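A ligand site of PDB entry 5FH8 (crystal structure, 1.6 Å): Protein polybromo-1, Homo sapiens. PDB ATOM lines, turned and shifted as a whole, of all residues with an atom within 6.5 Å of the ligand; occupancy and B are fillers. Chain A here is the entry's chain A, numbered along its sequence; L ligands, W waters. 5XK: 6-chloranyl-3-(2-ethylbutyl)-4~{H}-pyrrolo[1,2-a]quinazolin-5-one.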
ATOM      1  N   ILE A  41     -27.013  -3.981  23.208  1.00  0.00           N
ATOM      2  CA  ILE A  41     -27.253  -5.219  22.462  1.00  0.00           C
ATOM      3  C   ILE A  41     -25.980  -5.955  22.043  1.00  0.00           C
ATOM      4  O   ILE A  41     -26.028  -7.156  21.717  1.00  0.00           O
ATOM      5  CB  ILE A  41     -28.196  -4.952  21.254  1.00  0.00           C
ATOM      6  CG1 ILE A  41     -28.901  -6.196  20.722  1.00  0.00           C
ATOM      7  CG2 ILE A  41     -27.510  -4.133  20.188  1.00  0.00           C
ATOM      8  CD1 ILE A  41     -30.092  -5.857  19.853  1.00  0.00           C
ATOM      9  N   PHE A  42     -24.866  -5.234  22.004  1.00  0.00           N
ATOM     10  CA  PHE A  42     -23.590  -5.750  21.489  1.00  0.00           C
ATOM     11  C   PHE A  42     -22.670  -6.400  22.521  1.00  0.00           C
ATOM     12  O   PHE A  42     -21.588  -6.935  22.199  1.00  0.00           O
ATOM     13  CB  PHE A  42     -22.776  -4.674  20.771  1.00  0.00           C
ATOM     14  CG  PHE A  42     -23.477  -4.108  19.531  1.00  0.00           C
ATOM     15  CD1 PHE A  42     -23.433  -4.774  18.321  1.00  0.00           C
ATOM     16  CD2 PHE A  42     -24.165  -2.929  19.616  1.00  0.00           C
ATOM     17  CE1 PHE A  42     -24.102  -4.257  17.214  1.00  0.00           C
ATOM     18  CE2 PHE A  42     -24.855  -2.392  18.491  1.00  0.00           C
ATOM     19  CZ  PHE A  42     -24.843  -3.060  17.319  1.00  0.00           C
ATOM     20  N   LEU A  43     -23.047  -6.299  23.796  1.00  0.00           N
ATOM     21  CA  LEU A  43     -22.180  -6.915  24.849  1.00  0.00           C
ATOM     22  C   LEU A  43     -21.983  -8.399  24.662  1.00  0.00           C
ATOM     23  O   LEU A  43     -20.875  -8.892  24.801  1.00  0.00           O
ATOM     24  CB  LEU A  43     -22.750  -6.644  26.240  1.00  0.00           C
ATOM     25  CG  LEU A  43     -22.296  -5.392  26.890  1.00  0.00           C
ATOM     26  CD1 LEU A  43     -20.832  -5.601  27.343  1.00  0.00           C
ATOM     27  CD2 LEU A  43     -22.248  -4.180  25.999  1.00  0.00           C
ATOM     28  N   ARG A  44     -23.048  -9.128  24.328  1.00  0.00           N
ATOM     29  CA  ARG A  44     -23.069 -10.584  24.310  1.00  0.00           C
ATOM     30  C   ARG A  44     -23.764 -11.177  23.109  1.00  0.00           C
ATOM     31  O   ARG A  44     -24.930 -10.910  22.889  1.00  0.00           O
ATOM     32  CB  ARG A  44     -23.768 -11.093  25.599  1.00  0.00           C
ATOM     33  CG  ARG A  44     -23.594 -12.612  25.730  1.00  0.00           C
ATOM     34  CD  ARG A  44     -24.060 -13.155  27.061  1.00  0.00           C
ATOM     35  NE  ARG A  44     -23.349 -12.554  28.114  1.00  0.00           N
ATOM     36  CZ  ARG A  44     -23.772 -12.468  29.365  1.00  0.00           C
ATOM     37  NH1 ARG A  44     -24.855 -13.128  29.752  1.00  0.00           N
ATOM     38  NH2 ARG A  44     -23.050 -11.793  30.215  1.00  0.00           N
ATOM     39  N   LEU A  45     -23.033 -11.940  22.298  1.00  0.00           N
ATOM     40  CA  LEU A  45     -23.586 -12.644  21.183  1.00  0.00           C
ATOM     41  C   LEU A  45     -24.227 -13.930  21.706  1.00  0.00           C
ATOM     42  O   LEU A  45     -23.663 -14.557  22.622  1.00  0.00           O
ATOM     43  CB  LEU A  45     -22.468 -12.992  20.201  1.00  0.00           C
ATOM     44  CG  LEU A  45     -22.838 -13.568  18.839  1.00  0.00           C
ATOM     45  CD1 LEU A  45     -23.570 -12.545  18.006  1.00  0.00           C
ATOM     46  CD2 LEU A  45     -21.595 -14.084  18.123  1.00  0.00           C
ATOM     47  N   PRO A  46     -25.377 -14.363  21.156  1.00  0.00           N
ATOM     48  CA  PRO A  46     -25.913 -15.680  21.575  1.00  0.00           C
ATOM     49  C   PRO A  46     -24.968 -16.815  21.259  1.00  0.00           C
ATOM     50  O   PRO A  46     -24.153 -16.678  20.361  1.00  0.00           O
ATOM     51  CB  PRO A  46     -27.223 -15.814  20.809  1.00  0.00           C
ATOM     52  CG  PRO A  46     -27.526 -14.465  20.348  1.00  0.00           C
ATOM     53  CD  PRO A  46     -26.255 -13.706  20.204  1.00  0.00           C
ATOM     54  N   LEU A  51     -28.146 -19.760  18.418  1.00  0.00           N
ATOM     55  CA  LEU A  51     -28.232 -19.029  17.180  1.00  0.00           C
ATOM     56  C   LEU A  51     -27.213 -19.629  16.187  1.00  0.00           C
ATOM     57  O   LEU A  51     -26.287 -18.975  15.720  1.00  0.00           O
ATOM     58  CB  LEU A  51     -27.993 -17.542  17.414  1.00  0.00           C
ATOM     59  CG  LEU A  51     -28.488 -16.649  16.273  1.00  0.00           C
ATOM     60  CD1 LEU A  51     -30.011 -16.572  16.228  1.00  0.00           C
ATOM     61  CD2 LEU A  51     -27.879 -15.255  16.427  1.00  0.00           C
ATOM     62  N   TYR A  54     -25.942 -18.034  12.809  1.00  0.00           N
ATOM     63  CA  TYR A  54     -25.013 -16.854  12.868  1.00  0.00           C
ATOM     64  C   TYR A  54     -23.597 -17.351  12.604  1.00  0.00           C
ATOM     65  O   TYR A  54     -22.815 -16.776  11.853  1.00  0.00           O
ATOM     66  CB  TYR A  54     -25.076 -16.248  14.237  1.00  0.00           C
ATOM     67  CG  TYR A  54     -24.425 -14.892  14.339  1.00  0.00           C
ATOM     68  CD1 TYR A  54     -23.069 -14.735  14.574  1.00  0.00           C
ATOM     69  CD2 TYR A  54     -25.198 -13.739  14.183  1.00  0.00           C
ATOM     70  CE1 TYR A  54     -22.487 -13.458  14.652  1.00  0.00           C
ATOM     71  CE2 TYR A  54     -24.613 -12.466  14.225  1.00  0.00           C
ATOM     72  CZ  TYR A  54     -23.279 -12.328  14.506  1.00  0.00           C
ATOM     73  OH  TYR A  54     -22.720 -11.046  14.601  1.00  0.00           O
ATOM     74  N   ILE A  58     -21.162 -15.999   9.656  1.00  0.00           N
ATOM     75  CA  ILE A  58     -20.226 -15.019  10.181  1.00  0.00           C
ATOM     76  C   ILE A  58     -18.956 -15.722  10.628  1.00  0.00           C
ATOM     77  O   ILE A  58     -18.971 -16.488  11.600  1.00  0.00           O
ATOM     78  CB  ILE A  58     -20.864 -14.244  11.363  1.00  0.00           C
ATOM     79  CG1 ILE A  58     -22.231 -13.603  10.917  1.00  0.00           C
ATOM     80  CG2 ILE A  58     -19.848 -13.287  11.989  1.00  0.00           C
ATOM     81  CD1 ILE A  58     -22.101 -12.425   9.895  1.00  0.00           C
ATOM     82  N   MET A  62     -17.889 -12.003  17.184  1.00  0.00           N
ATOM     83  CA  MET A  62     -17.277 -10.980  18.068  1.00  0.00           C
ATOM     84  C   MET A  62     -18.359 -10.274  18.838  1.00  0.00           C
ATOM     85  O   MET A  62     -19.454 -10.051  18.348  1.00  0.00           O
ATOM     86  CB  MET A  62     -16.521  -9.986  17.161  1.00  0.00           C
ATOM     87  CG  MET A  62     -15.638  -9.021  17.877  1.00  0.00           C
ATOM     88  SD  MET A  62     -14.353  -9.770  18.923  1.00  0.00           S
ATOM     89  CE  MET A  62     -13.488 -10.553  17.617  1.00  0.00           C
ATOM     90  N   ASP A  63     -18.098 -10.039  20.140  1.00  0.00           N
ATOM     91  CA  ASP A  63     -18.965  -9.235  20.971  1.00  0.00           C
ATOM     92  C   ASP A  63     -18.115  -8.391  21.890  1.00  0.00           C
ATOM     93  O   ASP A  63     -16.863  -8.527  21.931  1.00  0.00           O
ATOM     94  CB  ASP A  63     -20.050 -10.052  21.687  1.00  0.00           C
ATOM     95  CG  ASP A  63     -19.518 -11.058  22.678  1.00  0.00           C
ATOM     96  OD1 ASP A  63     -18.377 -10.883  23.176  1.00  0.00           O
ATOM     97  OD2 ASP A  63     -20.268 -12.030  22.981  1.00  0.00           O
ATOM     98  N   MET A  64     -18.734  -7.438  22.574  1.00  0.00           N
ATOM     99  CA  MET A  64     -17.923  -6.501  23.383  1.00  0.00           C
ATOM    100  C   MET A  64     -17.355  -7.175  24.628  1.00  0.00           C
ATOM    101  O   MET A  64     -16.246  -6.792  25.038  1.00  0.00           O
ATOM    102  CB  MET A  64     -18.713  -5.237  23.734  1.00  0.00           C
ATOM    103  CG  MET A  64     -18.864  -4.368  22.527  1.00  0.00           C
ATOM    104  SD  MET A  64     -19.841  -2.878  22.820  1.00  0.00           S
ATOM    105  CE  MET A  64     -18.826  -2.026  23.951  1.00  0.00           C
ATOM    106  N   MET A  88     -14.874  -5.242  12.936  1.00  0.00           N
ATOM    107  CA  MET A  88     -15.374  -6.584  12.560  1.00  0.00           C
ATOM    108  C   MET A  88     -16.746  -6.852  13.152  1.00  0.00           C
ATOM    109  O   MET A  88     -17.668  -7.330  12.440  1.00  0.00           O
ATOM    110  CB  MET A  88     -14.367  -7.663  12.872  1.00  0.00           C
ATOM    111  CG  MET A  88     -14.845  -9.053  12.621  1.00  0.00           C
ATOM    112  SD  MET A  88     -14.798  -9.486  10.870  1.00  0.00           S
ATOM    113  CE  MET A  88     -13.020  -9.597  10.637  1.00  0.00           C
ATOM    114  N   MET A  89     -16.886  -6.594  14.465  1.00  0.00           N
ATOM    115  CA  MET A  89     -18.158  -6.777  15.152  1.00  0.00           C
ATOM    116  C   MET A  89     -19.293  -5.976  14.469  1.00  0.00           C
ATOM    117  O   MET A  89     -20.374  -6.490  14.223  1.00  0.00           O
ATOM    118  CB  MET A  89     -18.003  -6.348  16.624  1.00  0.00           C
ATOM    119  CG  MET A  89     -19.203  -6.587  17.386  1.00  0.00           C
ATOM    120  SD  MET A  89     -19.123  -6.009  19.097  1.00  0.00           S
ATOM    121  CE  MET A  89     -19.342  -4.243  18.819  1.00  0.00           C
ATOM    122  N   PHE A  90     -19.068  -4.704  14.126  1.00  0.00           N
ATOM    123  CA  PHE A  90     -20.145  -3.909  13.526  1.00  0.00           C
ATOM    124  C   PHE A  90     -20.438  -4.332  12.086  1.00  0.00           C
ATOM    125  O   PHE A  90     -21.617  -4.368  11.696  1.00  0.00           O
ATOM    126  CB  PHE A  90     -19.818  -2.415  13.625  1.00  0.00           C
ATOM    127  CG  PHE A  90     -19.752  -1.947  15.040  1.00  0.00           C
ATOM    128  CD1 PHE A  90     -20.780  -2.172  15.907  1.00  0.00           C
ATOM    129  CD2 PHE A  90     -18.693  -1.159  15.462  1.00  0.00           C
ATOM    130  CE1 PHE A  90     -20.788  -1.691  17.214  1.00  0.00           C
ATOM    131  CE2 PHE A  90     -18.657  -0.715  16.790  1.00  0.00           C
ATOM    132  CZ  PHE A  90     -19.682  -0.939  17.643  1.00  0.00           C
ATOM    133  N   ASN A  91     -19.421  -4.728  11.371  1.00  0.00           N
ATOM    134  CA  ASN A  91     -19.642  -5.337  10.028  1.00  0.00           C
ATOM    135  C   ASN A  91     -20.390  -6.642  10.076  1.00  0.00           C
ATOM    136  O   ASN A  91     -21.274  -6.872   9.262  1.00  0.00           O
ATOM    137  CB  ASN A  91     -18.295  -5.517   9.292  1.00  0.00           C
ATOM    138  CG  ASN A  91     -17.679  -4.165   8.847  1.00  0.00           C
ATOM    139  OD1 ASN A  91     -18.334  -3.148   8.728  1.00  0.00           O
ATOM    140  ND2 ASN A  91     -16.423  -4.217   8.520  1.00  0.00           N
ATOM    141  N   ASN A  92     -20.095  -7.495  11.073  1.00  0.00           N
ATOM    142  CA  ASN A  92     -20.823  -8.710  11.266  1.00  0.00           C
ATOM    143  C   ASN A  92     -22.263  -8.362  11.525  1.00  0.00           C
ATOM    144  O   ASN A  92     -23.157  -9.019  10.996  1.00  0.00           O
ATOM    145  CB  ASN A  92     -20.297  -9.497  12.476  1.00  0.00           C
ATOM    146  CG  ASN A  92     -18.940 -10.108  12.295  1.00  0.00           C
ATOM    147  OD1 ASN A  92     -18.413 -10.232  11.170  1.00  0.00           O
ATOM    148  ND2 ASN A  92     -18.370 -10.555  13.402  1.00  0.00           N
ATOM    149  N   ALA A  93     -22.558  -7.412  12.385  1.00  0.00           N
ATOM    150  CA  ALA A  93     -23.987  -7.048  12.654  1.00  0.00           C
ATOM    151  C   ALA A  93     -24.726  -6.597  11.429  1.00  0.00           C
ATOM    152  O   ALA A  93     -25.895  -6.951  11.232  1.00  0.00           O
ATOM    153  CB  ALA A  93     -24.076  -5.950  13.719  1.00  0.00           C
ATOM    154  N   CYS A  94     -24.033  -5.864  10.554  1.00  0.00           N
ATOM    155  CA  CYS A  94     -24.624  -5.317   9.326  1.00  0.00           C
ATOM    156  C   CYS A  94     -24.705  -6.299   8.206  1.00  0.00           C
ATOM    157  O   CYS A  94     -25.213  -5.965   7.127  1.00  0.00           O
ATOM    158  CB  CYS A  94     -23.881  -4.043   8.901  1.00  0.00           C
ATOM    159  SG  CYS A  94     -24.204  -2.661  10.010  1.00  0.00           S
ATOM    160  N   TYR A  96     -25.245  -9.936   9.133  1.00  0.00           N
ATOM    161  CA  TYR A  96     -26.259 -10.912   9.581  1.00  0.00           C
ATOM    162  C   TYR A  96     -27.675 -10.339   9.633  1.00  0.00           C
ATOM    163  O   TYR A  96     -28.681 -11.035   9.319  1.00  0.00           O
ATOM    164  CB  TYR A  96     -25.862 -11.470  10.959  1.00  0.00           C
ATOM    165  CG  TYR A  96     -26.831 -12.474  11.471  1.00  0.00           C
ATOM    166  CD1 TYR A  96     -26.774 -13.775  11.037  1.00  0.00           C
ATOM    167  CD2 TYR A  96     -27.773 -12.115  12.423  1.00  0.00           C
ATOM    168  CE1 TYR A  96     -27.641 -14.710  11.544  1.00  0.00           C
ATOM    169  CE2 TYR A  96     -28.680 -13.060  12.900  1.00  0.00           C
ATOM    170  CZ  TYR A  96     -28.583 -14.348  12.431  1.00  0.00           C
ATOM    171  OH  TYR A  96     -29.447 -15.309  12.879  1.00  0.00           O
ATOM    172  N   ASN A  97     -27.773  -9.065  10.036  1.00  0.00           N
ATOM    173  CA  ASN A  97     -29.045  -8.375  10.223  1.00  0.00           C
ATOM    174  C   ASN A  97     -29.372  -7.474   9.006  1.00  0.00           C
ATOM    175  O   ASN A  97     -28.490  -6.921   8.410  1.00  0.00           O
ATOM    176  CB  ASN A  97     -29.011  -7.565  11.548  1.00  0.00           C
ATOM    177  CG  ASN A  97     -28.743  -8.460  12.768  1.00  0.00           C
ATOM    178  OD1 ASN A  97     -29.643  -9.149  13.224  1.00  0.00           O
ATOM    179  ND2 ASN A  97     -27.517  -8.476  13.251  1.00  0.00           N
ATOM    180  N   SER A 101     -33.368  -3.321  10.025  1.00  0.00           N
ATOM    181  CA  SER A 101     -33.393  -3.644  11.444  1.00  0.00           C
ATOM    182  C   SER A 101     -32.817  -2.539  12.311  1.00  0.00           C
ATOM    183  O   SER A 101     -31.873  -1.843  11.936  1.00  0.00           O
ATOM    184  CB  SER A 101     -32.654  -4.967  11.736  1.00  0.00           C
ATOM    185  OG  SER A 101     -31.218  -4.851  11.473  1.00  0.00           O
ATOM    186  N   ILE A 103     -30.778  -3.051  14.910  1.00  0.00           N
ATOM    187  CA  ILE A 103     -29.391  -3.338  15.228  1.00  0.00           C
ATOM    188  C   ILE A 103     -28.441  -2.935  14.096  1.00  0.00           C
ATOM    189  O   ILE A 103     -27.332  -2.480  14.358  1.00  0.00           O
ATOM    190  CB  ILE A 103     -29.171  -4.801  15.681  1.00  0.00           C
ATOM    191  CG1 ILE A 103     -27.795  -5.004  16.246  1.00  0.00           C
ATOM    192  CG2 ILE A 103     -29.527  -5.767  14.545  1.00  0.00           C
ATOM    193  CD1 ILE A 103     -27.540  -6.407  16.759  1.00  0.00           C
HETATM  194  C4  5XK L   1     -31.494  -7.795  17.365  1.00  0.00           C
HETATM  195  C14 5XK L   1     -24.511  -9.151  17.342  1.00  0.00           C
HETATM  196  C5  5XK L   1     -29.538 -10.019  16.605  1.00  0.00           C
HETATM  197  C6  5XK L   1     -28.598  -9.993  17.534  1.00  0.00           C
HETATM  198  C11 5XK L   1     -23.213  -8.941  19.846  1.00  0.00           C
HETATM  199  C7  5XK L   1     -28.768 -10.178  19.012  1.00  0.00           C
HETATM  200  C8  5XK L   1     -27.431  -9.834  19.643  1.00  0.00           C
HETATM  201  C9  5XK L   1     -25.174  -9.390  18.565  1.00  0.00           C
HETATM  202  C10 5XK L   1     -24.541  -9.278  19.793  1.00  0.00           C
HETATM  203  C12 5XK L   1     -22.512  -8.694  18.666  1.00  0.00           C
HETATM  204  C13 5XK L   1     -23.163  -8.777  17.450  1.00  0.00           C
HETATM  205  N1  5XK L   1     -26.626  -9.555  16.135  1.00  0.00           N
HETATM  206  C3  5XK L   1     -31.780  -8.977  16.448  1.00  0.00           C
HETATM  207 CL   5XK L   1     -22.250  -8.186  16.069  1.00  0.00          CL
HETATM  208  C15 5XK L   1     -25.264  -9.281  16.068  1.00  0.00           C
HETATM  209  O   5XK L   1     -24.700  -9.263  14.987  1.00  0.00           O
HETATM  210  C16 5XK L   1     -27.209  -9.750  17.290  1.00  0.00           C
HETATM  211  N   5XK L   1     -26.537  -9.707  18.500  1.00  0.00           N
HETATM  212  C2  5XK L   1     -31.016 -10.217  16.813  1.00  0.00           C
HETATM  213  C1  5XK L   1     -31.406 -11.390  15.876  1.00  0.00           C
HETATM  214  C   5XK L   1     -30.899 -12.715  16.362  1.00  0.00           C
HETATM  215  O   HOH W   1     -20.142 -10.795  15.735  1.00  0.00           O
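The side-chain hydroxyl (OH) of Tyr 54 lies within hydrogen-bond range of an oxygen (O) of the ligand, 2.7 Å away. ND2 of Asn 97 sits close to N1 of the ligand (3.2 Å).
The backbone NH of Met 64 is in hydrogen-bond range of the side-chain sulfur of Met 89. The backbone carbonyl oxygen of Ala 93 lies within hydrogen-bond range of the side-chain amide nitrogen of Asn 97. The backbone NH (N) of Met 64 is in hydrogen-bond range of the backbone carbonyl oxygen (O) of Phe 42. The backbone NH (N) of Leu 45 is in hydrogen-bond range of the side-chain carboxylate (OD2) of Asp 63.
Ile 41 touches the ligand (O to C10, 3.2 Å). Phe 42 touches the ligand. Arg 44 touches the ligand (O to C10, 3.5 Å). CD1 of Leu 45 touches C9 of the ligand (3.6 Å). Leu 51 touches the ligand (CD2 to C, 3.9 Å). Met 62 touches the ligand (O to C12, 3.4 Å). Asp 63 touches the ligand. Met 89 touches the ligand (O to CL, 3.1 Å). Ala 93 touches the ligand (CA to O, 3.3 Å). CD1 of Ile 103 touches N1 of the ligand, 3.3 Å away. The nearest printed residue that does not touch the ligand is Pro 46 (4.1 Å).
Water W1 lies within hydrogen-bond range of O of Met 62 (2.8 Å), OH of Tyr 54 (2.8 Å) and ND2 of Asn 92 (2.9 Å).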
